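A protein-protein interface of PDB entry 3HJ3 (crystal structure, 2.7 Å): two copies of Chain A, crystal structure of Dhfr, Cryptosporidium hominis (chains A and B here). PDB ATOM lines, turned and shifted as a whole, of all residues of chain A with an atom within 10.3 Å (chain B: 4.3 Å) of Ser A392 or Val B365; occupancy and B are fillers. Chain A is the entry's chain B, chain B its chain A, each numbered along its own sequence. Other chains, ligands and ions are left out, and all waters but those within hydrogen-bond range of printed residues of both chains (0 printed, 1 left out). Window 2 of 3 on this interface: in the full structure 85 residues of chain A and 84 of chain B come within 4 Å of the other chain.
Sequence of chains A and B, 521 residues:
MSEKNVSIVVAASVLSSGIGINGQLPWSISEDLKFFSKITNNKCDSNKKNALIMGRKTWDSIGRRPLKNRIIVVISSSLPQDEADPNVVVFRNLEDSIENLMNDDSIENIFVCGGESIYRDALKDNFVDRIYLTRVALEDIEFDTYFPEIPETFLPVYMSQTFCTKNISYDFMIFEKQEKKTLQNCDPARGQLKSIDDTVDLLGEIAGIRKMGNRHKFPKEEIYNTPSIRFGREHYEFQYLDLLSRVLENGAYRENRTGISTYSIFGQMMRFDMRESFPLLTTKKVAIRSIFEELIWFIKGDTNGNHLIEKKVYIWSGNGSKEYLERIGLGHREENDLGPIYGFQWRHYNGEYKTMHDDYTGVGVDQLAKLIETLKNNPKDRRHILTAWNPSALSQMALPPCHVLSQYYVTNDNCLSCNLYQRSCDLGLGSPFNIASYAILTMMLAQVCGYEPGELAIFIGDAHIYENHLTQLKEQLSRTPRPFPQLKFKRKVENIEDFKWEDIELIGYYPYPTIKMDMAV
The side-chain hydroxyl (OH) of Tyr B349 sits at hydrogen-bond distance from the side-chain hydroxyl (OH) of Tyr A349, 2.6 Å away. The side-chain amide oxygen of Asn B350 sits at hydrogen-bond distance from the side-chain amide nitrogen of Asn A350 (2.6 Å). ND2 of Asn B350 lies within hydrogen-bond range of OD1 of Asn A390. ND2 of Asn B350 is in hydrogen-bond range of OG of Ser A392 (3.0 Å).
The backbone carbonyl oxygen (O) of Val B365 lies within hydrogen-bond range of the backbone NH (N) of Tyr B349 (2.8 Å). The backbone NH of Tyr A349 sits at hydrogen-bond distance from the backbone carbonyl oxygen of Phe A344 (3.5 Å). The side-chain amide oxygen (OE1) of Gln A345 lies within hydrogen-bond range of the side-chain amide nitrogen (ND2) of Asn A390 (3.0 Å). OH of Tyr A349 lies within hydrogen-bond range of O of Trp A389 (3.4 Å). OD1 of Asn A350 sits at hydrogen-bond distance from ND2 of Asn A390. The side-chain amide oxygen (OD1) of Asn A390 lies within hydrogen-bond range of the backbone NH (N) of Ser A392.
Pro A391 touches Tyr B349 (CG to CD2, 3.5 Å). CG of Pro A391 touches OE1 of Gln B367, 3.9 Å away. Ser A392 touches Val B365 (OG to CG2, 3.8 Å).
Printed residues of chain B within 4 Å of Asn A350: Asn B350. Printed residues of chain B within 4 Å of Pro A391: Tyr B349 (3.5 Å) and Gln B367 (3.9 Å). Of chain B, only Asn B350 (3.0 Å) and Val B365 (3.8 Å) come within 4 Å of Ser A392. Printed residues of chain A within 4 Å of Tyr B349: Tyr A349 and Pro A391. Asn B350 touches just these residues of chain A: Asn A350 (2.6 Å), Asn A390 (3.4 Å) and Ser A392 (3.0 Å). No residue of chain A comes within 4 Å of Gly B364. Asp B366 touches none of the printed residues of chain A. The nearest printed residue of chain B that does not touch Ser A392 is Tyr B349 (4.7 Å). The nearest residue of chain A that does not touch Val B365 is Pro A391 (4.2 Å).
Hydrophobic or aromatic side chains of chain B within 4 Å of the printed part of chain A: Tyr B349 and Val B365. Along chain B the printed residues that touch a printed residue of chain A span positions 349 to 367. Of the 22 printed residues of chain A, 5 touch a printed residue of chain B. Printed residues of chain A that touch a printed residue of chain B: Tyr A349, Asn A350, Asn A390, Pro A391 and Ser A392. Hydrophobic or aromatic side chains of chain A that line the printed part of chain B: Tyr A349 and Pro A391. Along chain A the printed residues that touch a printed residue of chain B span positions 349 to 392.
Tyr B349 touches its own counterpart, Tyr A349. Asn B350 touches its own counterpart, Asn A350. Positions printed for both chains: 348, 349 and 350. Of the 7 pairs that touch across the chains among the printed residues, 2 have their exchanged pair printed and touching as well.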
ATOM      1  N   ARG A 333     -28.465  -2.814 -20.156  1.00  0.00           N
ATOM      2  CA  ARG A 333     -28.540  -1.426 -20.610  1.00  0.00           C
ATOM      3  C   ARG A 333     -29.375  -1.272 -21.896  1.00  0.00           C
ATOM      4  O   ARG A 333     -29.299  -2.112 -22.814  1.00  0.00           O
ATOM      5  CB  ARG A 333     -27.119  -0.874 -20.780  1.00  0.00           C
ATOM      6  CG  ARG A 333     -27.011   0.645 -20.918  1.00  0.00           C
ATOM      7  CD  ARG A 333     -27.045   1.442 -19.592  1.00  0.00           C
ATOM      8  NE  ARG A 333     -25.820   1.362 -18.784  1.00  0.00           N
ATOM      9  CZ  ARG A 333     -24.608   1.808 -19.130  1.00  0.00           C
ATOM     10  NH1 ARG A 333     -24.383   2.355 -20.311  1.00  0.00           N
ATOM     11  NH2 ARG A 333     -23.594   1.676 -18.289  1.00  0.00           N
ATOM     12  N   PRO A 340     -21.486   6.741 -19.161  1.00  0.00           N
ATOM     13  CA  PRO A 340     -20.902   8.040 -18.860  1.00  0.00           C
ATOM     14  C   PRO A 340     -19.562   8.201 -19.606  1.00  0.00           C
ATOM     15  O   PRO A 340     -18.487   8.370 -18.997  1.00  0.00           O
ATOM     16  CB  PRO A 340     -20.741   7.999 -17.346  1.00  0.00           C
ATOM     17  CG  PRO A 340     -20.492   6.534 -17.058  1.00  0.00           C
ATOM     18  CD  PRO A 340     -21.267   5.746 -18.098  1.00  0.00           C
ATOM     19  N   PHE A 344     -20.527  13.057 -20.767  1.00  0.00           N
ATOM     20  CA  PHE A 344     -20.894  12.905 -19.377  1.00  0.00           C
ATOM     21  C   PHE A 344     -19.738  13.411 -18.495  1.00  0.00           C
ATOM     22  O   PHE A 344     -19.951  14.249 -17.603  1.00  0.00           O
ATOM     23  CB  PHE A 344     -21.337  11.508 -18.953  1.00  0.00           C
ATOM     24  CG  PHE A 344     -22.091  11.525 -17.613  1.00  0.00           C
ATOM     25  CD1 PHE A 344     -21.419  11.261 -16.410  1.00  0.00           C
ATOM     26  CD2 PHE A 344     -23.442  11.905 -17.560  1.00  0.00           C
ATOM     27  CE1 PHE A 344     -22.086  11.337 -15.187  1.00  0.00           C
ATOM     28  CE2 PHE A 344     -24.140  11.989 -16.326  1.00  0.00           C
ATOM     29  CZ  PHE A 344     -23.471  11.702 -15.155  1.00  0.00           C
ATOM     30  N   GLN A 345     -18.515  12.954 -18.765  1.00  0.00           N
ATOM     31  CA  GLN A 345     -17.386  13.414 -17.950  1.00  0.00           C
ATOM     32  C   GLN A 345     -17.088  14.923 -18.150  1.00  0.00           C
ATOM     33  O   GLN A 345     -16.687  15.628 -17.188  1.00  0.00           O
ATOM     34  CB  GLN A 345     -16.159  12.559 -18.196  1.00  0.00           C
ATOM     35  CG  GLN A 345     -16.399  11.048 -18.024  1.00  0.00           C
ATOM     36  CD  GLN A 345     -16.852  10.637 -16.579  1.00  0.00           C
ATOM     37  OE1 GLN A 345     -16.377  11.189 -15.546  1.00  0.00           O
ATOM     38  NE2 GLN A 345     -17.760   9.640 -16.515  1.00  0.00           N
ATOM     39  N   HIS A 348     -20.496  16.362 -16.268  1.00  0.00           N
ATOM     40  CA  HIS A 348     -20.970  15.812 -15.008  1.00  0.00           C
ATOM     41  C   HIS A 348     -19.929  14.860 -14.521  1.00  0.00           C
ATOM     42  O   HIS A 348     -20.240  13.734 -14.122  1.00  0.00           O
ATOM     43  CB  HIS A 348     -22.337  15.115 -15.151  1.00  0.00           C
ATOM     44  CG  HIS A 348     -23.320  15.856 -16.020  1.00  0.00           C
ATOM     45  ND1 HIS A 348     -23.942  17.024 -15.618  1.00  0.00           N
ATOM     46  CD2 HIS A 348     -23.801  15.590 -17.264  1.00  0.00           C
ATOM     47  CE1 HIS A 348     -24.742  17.462 -16.582  1.00  0.00           C
ATOM     48  NE2 HIS A 348     -24.688  16.603 -17.585  1.00  0.00           N
ATOM     49  N   TYR A 349     -18.690  15.338 -14.550  1.00  0.00           N
ATOM     50  CA  TYR A 349     -17.543  14.572 -14.055  1.00  0.00           C
ATOM     51  C   TYR A 349     -17.905  13.977 -12.729  1.00  0.00           C
ATOM     52  O   TYR A 349     -18.286  14.708 -11.818  1.00  0.00           O
ATOM     53  CB  TYR A 349     -16.266  15.439 -13.856  1.00  0.00           C
ATOM     54  CG  TYR A 349     -15.083  14.557 -13.623  1.00  0.00           C
ATOM     55  CD1 TYR A 349     -14.469  13.894 -14.691  1.00  0.00           C
ATOM     56  CD2 TYR A 349     -14.647  14.276 -12.325  1.00  0.00           C
ATOM     57  CE1 TYR A 349     -13.421  12.994 -14.464  1.00  0.00           C
ATOM     58  CE2 TYR A 349     -13.602  13.368 -12.075  1.00  0.00           C
ATOM     59  CZ  TYR A 349     -12.990  12.733 -13.143  1.00  0.00           C
ATOM     60  OH  TYR A 349     -11.944  11.839 -12.959  1.00  0.00           O
ATOM     61  N   ASN A 350     -17.809  12.659 -12.621  1.00  0.00           N
ATOM     62  CA  ASN A 350     -18.066  11.981 -11.357  1.00  0.00           C
ATOM     63  C   ASN A 350     -19.486  11.931 -10.871  1.00  0.00           C
ATOM     64  O   ASN A 350     -19.721  11.483  -9.761  1.00  0.00           O
ATOM     65  CB  ASN A 350     -17.243  12.581 -10.235  1.00  0.00           C
ATOM     66  CG  ASN A 350     -16.036  11.741  -9.907  1.00  0.00           C
ATOM     67  OD1 ASN A 350     -15.934  10.546 -10.305  1.00  0.00           O
ATOM     68  ND2 ASN A 350     -15.080  12.363  -9.196  1.00  0.00           N
ATOM     69  N   GLY A 351     -20.436  12.397 -11.665  1.00  0.00           N
ATOM     70  CA  GLY A 351     -21.824  12.284 -11.258  1.00  0.00           C
ATOM     71  C   GLY A 351     -22.241  10.826 -11.309  1.00  0.00           C
ATOM     72  O   GLY A 351     -21.553  10.001 -11.910  1.00  0.00           O
ATOM     73  N   GLU A 352     -23.353  10.497 -10.654  1.00  0.00           N
ATOM     74  CA  GLU A 352     -23.793   9.115 -10.644  1.00  0.00           C
ATOM     75  C   GLU A 352     -24.552   8.798 -11.943  1.00  0.00           C
ATOM     76  O   GLU A 352     -25.563   9.439 -12.248  1.00  0.00           O
ATOM     77  CB  GLU A 352     -24.619   8.798  -9.395  1.00  0.00           C
ATOM     78  CG  GLU A 352     -24.909   7.277  -9.273  1.00  0.00           C
ATOM     79  CD  GLU A 352     -25.921   6.925  -8.177  1.00  0.00           C
ATOM     80  OE1 GLU A 352     -26.968   7.601  -8.060  1.00  0.00           O
ATOM     81  OE2 GLU A 352     -25.664   5.952  -7.441  1.00  0.00           O
ATOM     82  N   TYR A 353     -24.065   7.816 -12.700  1.00  0.00           N
ATOM     83  CA  TYR A 353     -24.756   7.421 -13.916  1.00  0.00           C
ATOM     84  C   TYR A 353     -25.995   6.501 -13.700  1.00  0.00           C
ATOM     85  O   TYR A 353     -25.862   5.295 -13.487  1.00  0.00           O
ATOM     86  CB  TYR A 353     -23.801   6.791 -14.928  1.00  0.00           C
ATOM     87  CG  TYR A 353     -24.383   6.806 -16.323  1.00  0.00           C
ATOM     88  CD1 TYR A 353     -24.503   8.008 -17.027  1.00  0.00           C
ATOM     89  CD2 TYR A 353     -24.853   5.638 -16.916  1.00  0.00           C
ATOM     90  CE1 TYR A 353     -25.078   8.046 -18.301  1.00  0.00           C
ATOM     91  CE2 TYR A 353     -25.416   5.644 -18.186  1.00  0.00           C
ATOM     92  CZ  TYR A 353     -25.529   6.864 -18.879  1.00  0.00           C
ATOM     93  OH  TYR A 353     -26.062   6.919 -20.148  1.00  0.00           O
ATOM     94  N   ALA A 388     -11.296  13.373 -19.273  1.00  0.00           N
ATOM     95  CA  ALA A 388     -12.352  12.390 -19.484  1.00  0.00           C
ATOM     96  C   ALA A 388     -11.981  11.043 -18.873  1.00  0.00           C
ATOM     97  O   ALA A 388     -12.813  10.141 -18.781  1.00  0.00           O
ATOM     98  CB  ALA A 388     -12.646  12.238 -20.969  1.00  0.00           C
ATOM     99  N   TRP A 389     -10.725  10.914 -18.455  1.00  0.00           N
ATOM    100  CA  TRP A 389     -10.261   9.705 -17.784  1.00  0.00           C
ATOM    101  C   TRP A 389     -10.736   9.662 -16.335  1.00  0.00           C
ATOM    102  O   TRP A 389     -10.181  10.341 -15.471  1.00  0.00           O
ATOM    103  CB  TRP A 389      -8.736   9.612 -17.842  1.00  0.00           C
ATOM    104  CG  TRP A 389      -8.207   8.245 -17.532  1.00  0.00           C
ATOM    105  CD1 TRP A 389      -7.534   7.862 -16.408  1.00  0.00           C
ATOM    106  CD2 TRP A 389      -8.306   7.079 -18.358  1.00  0.00           C
ATOM    107  NE1 TRP A 389      -7.208   6.530 -16.482  1.00  0.00           N
ATOM    108  CE2 TRP A 389      -7.670   6.025 -17.670  1.00  0.00           C
ATOM    109  CE3 TRP A 389      -8.868   6.823 -19.611  1.00  0.00           C
ATOM    110  CZ2 TRP A 389      -7.584   4.737 -18.193  1.00  0.00           C
ATOM    111  CZ3 TRP A 389      -8.782   5.543 -20.129  1.00  0.00           C
ATOM    112  CH2 TRP A 389      -8.144   4.516 -19.421  1.00  0.00           C
ATOM    113  N   ASN A 390     -11.762   8.859 -16.078  1.00  0.00           N
ATOM    114  CA  ASN A 390     -12.301   8.716 -14.738  1.00  0.00           C
ATOM    115  C   ASN A 390     -12.210   7.278 -14.281  1.00  0.00           C
ATOM    116  O   ASN A 390     -13.079   6.491 -14.626  1.00  0.00           O
ATOM    117  CB  ASN A 390     -13.751   9.137 -14.699  1.00  0.00           C
ATOM    118  CG  ASN A 390     -14.254   9.216 -13.302  1.00  0.00           C
ATOM    119  OD1 ASN A 390     -13.722   8.511 -12.427  1.00  0.00           O
ATOM    120  ND2 ASN A 390     -15.215  10.121 -13.033  1.00  0.00           N
ATOM    121  N   PRO A 391     -11.139   6.894 -13.559  1.00  0.00           N
ATOM    122  CA  PRO A 391     -11.048   5.484 -13.172  1.00  0.00           C
ATOM    123  C   PRO A 391     -12.318   4.931 -12.485  1.00  0.00           C
ATOM    124  O   PRO A 391     -12.652   3.762 -12.650  1.00  0.00           O
ATOM    125  CB  PRO A 391      -9.814   5.434 -12.248  1.00  0.00           C
ATOM    126  CG  PRO A 391      -9.328   6.863 -12.173  1.00  0.00           C
ATOM    127  CD  PRO A 391      -9.836   7.531 -13.407  1.00  0.00           C
ATOM    128  N   SER A 392     -13.053   5.773 -11.777  1.00  0.00           N
ATOM    129  CA  SER A 392     -14.288   5.292 -11.148  1.00  0.00           C
ATOM    130  C   SER A 392     -15.362   4.871 -12.102  1.00  0.00           C
ATOM    131  O   SER A 392     -16.248   4.114 -11.718  1.00  0.00           O
ATOM    132  CB  SER A 392     -14.855   6.328 -10.213  1.00  0.00           C
ATOM    133  OG  SER A 392     -14.165   6.202  -8.991  1.00  0.00           O
ATOM    134  N   ALA A 393     -15.292   5.339 -13.345  1.00  0.00           N
ATOM    135  CA  ALA A 393     -16.405   5.119 -14.247  1.00  0.00           C
ATOM    136  C   ALA A 393     -16.108   4.339 -15.499  1.00  0.00           C
ATOM    137  O   ALA A 393     -16.959   4.299 -16.388  1.00  0.00           O
ATOM    138  CB  ALA A 393     -17.077   6.440 -14.587  1.00  0.00           C
ATOM    139  N   LEU A 394     -14.939   3.711 -15.590  1.00  0.00           N
ATOM    140  CA  LEU A 394     -14.542   3.087 -16.866  1.00  0.00           C
ATOM    141  C   LEU A 394     -15.443   1.937 -17.205  1.00  0.00           C
ATOM    142  O   LEU A 394     -15.901   1.820 -18.331  1.00  0.00           O
ATOM    143  CB  LEU A 394     -13.083   2.608 -16.841  1.00  0.00           C
ATOM    144  CG  LEU A 394     -12.002   3.686 -16.601  1.00  0.00           C
ATOM    145  CD1 LEU A 394     -10.606   3.047 -16.480  1.00  0.00           C
ATOM    146  CD2 LEU A 394     -12.019   4.779 -17.690  1.00  0.00           C
ATOM    147  N   SER A 395     -15.707   1.097 -16.201  1.00  0.00           N
ATOM    148  CA  SER A 395     -16.498  -0.127 -16.355  1.00  0.00           C
ATOM    149  C   SER A 395     -17.921   0.098 -16.877  1.00  0.00           C
ATOM    150  O   SER A 395     -18.420  -0.704 -17.679  1.00  0.00           O
ATOM    151  CB  SER A 395     -16.541  -0.883 -15.033  1.00  0.00           C
ATOM    152  OG  SER A 395     -17.090  -0.060 -14.021  1.00  0.00           O
ATOM    153  N   GLN A 396     -18.570   1.181 -16.439  1.00  0.00           N
ATOM    154  CA  GLN A 396     -19.907   1.526 -16.931  1.00  0.00           C
ATOM    155  C   GLN A 396     -19.869   2.118 -18.325  1.00  0.00           C
ATOM    156  O   GLN A 396     -20.919   2.399 -18.888  1.00  0.00           O
ATOM    157  CB  GLN A 396     -20.569   2.533 -16.009  1.00  0.00           C
ATOM    158  CG  GLN A 396     -20.235   2.331 -14.559  1.00  0.00           C
ATOM    159  CD  GLN A 396     -21.338   2.836 -13.644  1.00  0.00           C
ATOM    160  OE1 GLN A 396     -21.575   4.046 -13.524  1.00  0.00           O
ATOM    161  NE2 GLN A 396     -22.021   1.902 -12.992  1.00  0.00           N
ATOM    162  N   MET A 397     -18.670   2.340 -18.869  1.00  0.00           N
ATOM    163  CA  MET A 397     -18.545   3.047 -20.137  1.00  0.00           C
ATOM    164  C   MET A 397     -18.550   2.065 -21.268  1.00  0.00           C
ATOM    165  O   MET A 397     -17.852   1.035 -21.204  1.00  0.00           O
ATOM    166  CB  MET A 397     -17.255   3.876 -20.202  1.00  0.00           C
ATOM    167  CG  MET A 397     -17.294   5.176 -19.450  1.00  0.00           C
ATOM    168  SD  MET A 397     -15.747   6.075 -19.616  1.00  0.00           S
ATOM    169  CE  MET A 397     -15.779   6.326 -21.370  1.00  0.00           C
ATOM    170  N   PRO A 400     -13.785   2.912 -22.903  1.00  0.00           N
ATOM    171  CA  PRO A 400     -12.951   3.873 -22.153  1.00  0.00           C
ATOM    172  C   PRO A 400     -12.374   4.886 -23.148  1.00  0.00           C
ATOM    173  O   PRO A 400     -11.941   4.485 -24.247  1.00  0.00           O
ATOM    174  CB  PRO A 400     -11.862   3.002 -21.538  1.00  0.00           C
ATOM    175  CG  PRO A 400     -12.363   1.594 -21.709  1.00  0.00           C
ATOM    176  CD  PRO A 400     -13.148   1.592 -22.973  1.00  0.00           C
ATOM    177  N   PRO A 401     -12.403   6.193 -22.780  1.00  0.00           N
ATOM    178  CA  PRO A 401     -12.016   7.309 -23.633  1.00  0.00           C
ATOM    179  C   PRO A 401     -10.587   7.196 -24.234  1.00  0.00           C
ATOM    180  O   PRO A 401      -9.630   6.720 -23.575  1.00  0.00           O
ATOM    181  CB  PRO A 401     -12.091   8.490 -22.668  1.00  0.00           C
ATOM    182  CG  PRO A 401     -11.826   7.922 -21.345  1.00  0.00           C
ATOM    183  CD  PRO A 401     -12.558   6.635 -21.378  1.00  0.00           C
ATOM    184  N   ARG B 347      -3.349   6.186  -5.172  1.00  0.00           N
ATOM    185  CA  ARG B 347      -3.738   4.990  -4.418  1.00  0.00           C
ATOM    186  C   ARG B 347      -5.176   5.060  -3.987  1.00  0.00           C
ATOM    187  O   ARG B 347      -5.786   4.033  -3.673  1.00  0.00           O
ATOM    188  CB  ARG B 347      -2.845   4.732  -3.196  1.00  0.00           C
ATOM    189  CG  ARG B 347      -1.322   4.835  -3.446  1.00  0.00           C
ATOM    190  CD  ARG B 347      -0.829   3.892  -4.556  1.00  0.00           C
ATOM    191  NE  ARG B 347      -1.228   2.528  -4.226  1.00  0.00           N
ATOM    192  CZ  ARG B 347      -0.682   1.810  -3.252  1.00  0.00           C
ATOM    193  NH1 ARG B 347       0.303   2.288  -2.537  1.00  0.00           N
ATOM    194  NH2 ARG B 347      -1.144   0.620  -2.982  1.00  0.00           N
ATOM    195  N   HIS B 348      -5.736   6.264  -4.005  1.00  0.00           N
ATOM    196  CA  HIS B 348      -7.096   6.458  -3.487  1.00  0.00           C
ATOM    197  C   HIS B 348      -7.939   7.337  -4.358  1.00  0.00           C
ATOM    198  O   HIS B 348      -8.709   8.169  -3.857  1.00  0.00           O
ATOM    199  CB  HIS B 348      -7.029   7.036  -2.069  1.00  0.00           C
ATOM    200  CG  HIS B 348      -6.219   6.204  -1.125  1.00  0.00           C
ATOM    201  ND1 HIS B 348      -6.515   4.881  -0.860  1.00  0.00           N
ATOM    202  CD2 HIS B 348      -5.123   6.505  -0.391  1.00  0.00           C
ATOM    203  CE1 HIS B 348      -5.630   4.402  -0.007  1.00  0.00           C
ATOM    204  NE2 HIS B 348      -4.777   5.370   0.300  1.00  0.00           N
ATOM    205  N   TYR B 349      -7.808   7.164  -5.671  1.00  0.00           N
ATOM    206  CA  TYR B 349      -8.538   8.004  -6.599  1.00  0.00           C
ATOM    207  C   TYR B 349      -9.999   8.126  -6.204  1.00  0.00           C
ATOM    208  O   TYR B 349     -10.709   7.118  -5.993  1.00  0.00           O
ATOM    209  CB  TYR B 349      -8.433   7.501  -8.026  1.00  0.00           C
ATOM    210  CG  TYR B 349      -8.829   8.589  -8.980  1.00  0.00           C
ATOM    211  CD1 TYR B 349      -7.883   9.494  -9.439  1.00  0.00           C
ATOM    212  CD2 TYR B 349     -10.153   8.773  -9.343  1.00  0.00           C
ATOM    213  CE1 TYR B 349      -8.220  10.510 -10.250  1.00  0.00           C
ATOM    214  CE2 TYR B 349     -10.514   9.793 -10.163  1.00  0.00           C
ATOM    215  CZ  TYR B 349      -9.538  10.669 -10.619  1.00  0.00           C
ATOM    216  OH  TYR B 349      -9.883  11.720 -11.449  1.00  0.00           O
ATOM    217  N   ASN B 350     -10.458   9.358  -6.104  1.00  0.00           N
ATOM    218  CA  ASN B 350     -11.878   9.660  -5.844  1.00  0.00           C
ATOM    219  C   ASN B 350     -12.293   9.483  -4.418  1.00  0.00           C
ATOM    220  O   ASN B 350     -13.432   9.793  -4.077  1.00  0.00           O
ATOM    221  CB  ASN B 350     -12.822   8.890  -6.747  1.00  0.00           C
ATOM    222  CG  ASN B 350     -13.279   9.717  -7.929  1.00  0.00           C
ATOM    223  OD1 ASN B 350     -13.514  10.912  -7.788  1.00  0.00           O
ATOM    224  ND2 ASN B 350     -13.412   9.084  -9.114  1.00  0.00           N
ATOM    225  N   GLY B 364     -11.407   4.432  -2.291  1.00  0.00           N
ATOM    226  CA  GLY B 364     -11.049   4.941  -3.592  1.00  0.00           C
ATOM    227  C   GLY B 364     -10.445   3.882  -4.479  1.00  0.00           C
ATOM    228  O   GLY B 364     -10.099   2.814  -4.005  1.00  0.00           O
ATOM    229  N   VAL B 365     -10.320   4.183  -5.767  1.00  0.00           N
ATOM    230  CA  VAL B 365      -9.609   3.310  -6.694  1.00  0.00           C
ATOM    231  C   VAL B 365      -8.104   3.365  -6.456  1.00  0.00           C
ATOM    232  O   VAL B 365      -7.509   4.442  -6.429  1.00  0.00           O
ATOM    233  CB  VAL B 365      -9.903   3.681  -8.158  1.00  0.00           C
ATOM    234  CG1 VAL B 365      -9.131   2.772  -9.101  1.00  0.00           C
ATOM    235  CG2 VAL B 365     -11.396   3.604  -8.436  1.00  0.00           C
ATOM    236  N   ASP B 366      -7.493   2.197  -6.286  1.00  0.00           N
ATOM    237  CA  ASP B 366      -6.046   2.062  -6.414  1.00  0.00           C
ATOM    238  C   ASP B 366      -5.630   1.959  -7.877  1.00  0.00           C
ATOM    239  O   ASP B 366      -5.601   0.869  -8.450  1.00  0.00           O
ATOM    240  CB  ASP B 366      -5.552   0.840  -5.639  1.00  0.00           C
ATOM    241  CG  ASP B 366      -4.124   0.996  -5.154  1.00  0.00           C
ATOM    242  OD1 ASP B 366      -3.799   0.457  -4.076  1.00  0.00           O
ATOM    243  OD2 ASP B 366      -3.327   1.656  -5.853  1.00  0.00           O
ATOM    244  N   GLN B 367      -5.308   3.101  -8.478  1.00  0.00           N
ATOM    245  CA  GLN B 367      -4.712   3.126  -9.808  1.00  0.00           C
ATOM    246  C   GLN B 367      -3.397   2.354  -9.837  1.00  0.00           C
ATOM    247  O   GLN B 367      -3.186   1.501 -10.699  1.00  0.00           O
ATOM    248  CB  GLN B 367      -4.486   4.568 -10.266  1.00  0.00           C
ATOM    249  CG  GLN B 367      -5.764   5.376 -10.427  1.00  0.00           C
ATOM    250  CD  GLN B 367      -5.524   6.721 -11.084  1.00  0.00           C
ATOM    251  OE1 GLN B 367      -5.445   6.821 -12.308  1.00  0.00           O
ATOM    252  NE2 GLN B 367      -5.405   7.763 -10.270  1.00  0.00           N
ATOM    253  N   LYS B 370      -3.815  -1.258  -9.709  1.00  0.00           N
ATOM    254  CA  LYS B 370      -4.374  -1.765 -10.982  1.00  0.00           C
ATOM    255  C   LYS B 370      -3.344  -1.659 -12.098  1.00  0.00           C
ATOM    256  O   LYS B 370      -3.359  -2.462 -13.049  1.00  0.00           O
ATOM    257  CB  LYS B 370      -5.657  -1.064 -11.404  1.00  0.00           C
ATOM    258  CG  LYS B 370      -6.797  -1.158 -10.378  1.00  0.00           C
ATOM    259  CD  LYS B 370      -8.135  -0.706 -11.022  1.00  0.00           C
ATOM    260  CE  LYS B 370      -9.311  -1.480 -10.422  1.00  0.00           C
ATOM    261  NZ  LYS B 370      -9.560  -1.053  -9.005  1.00  0.00           N
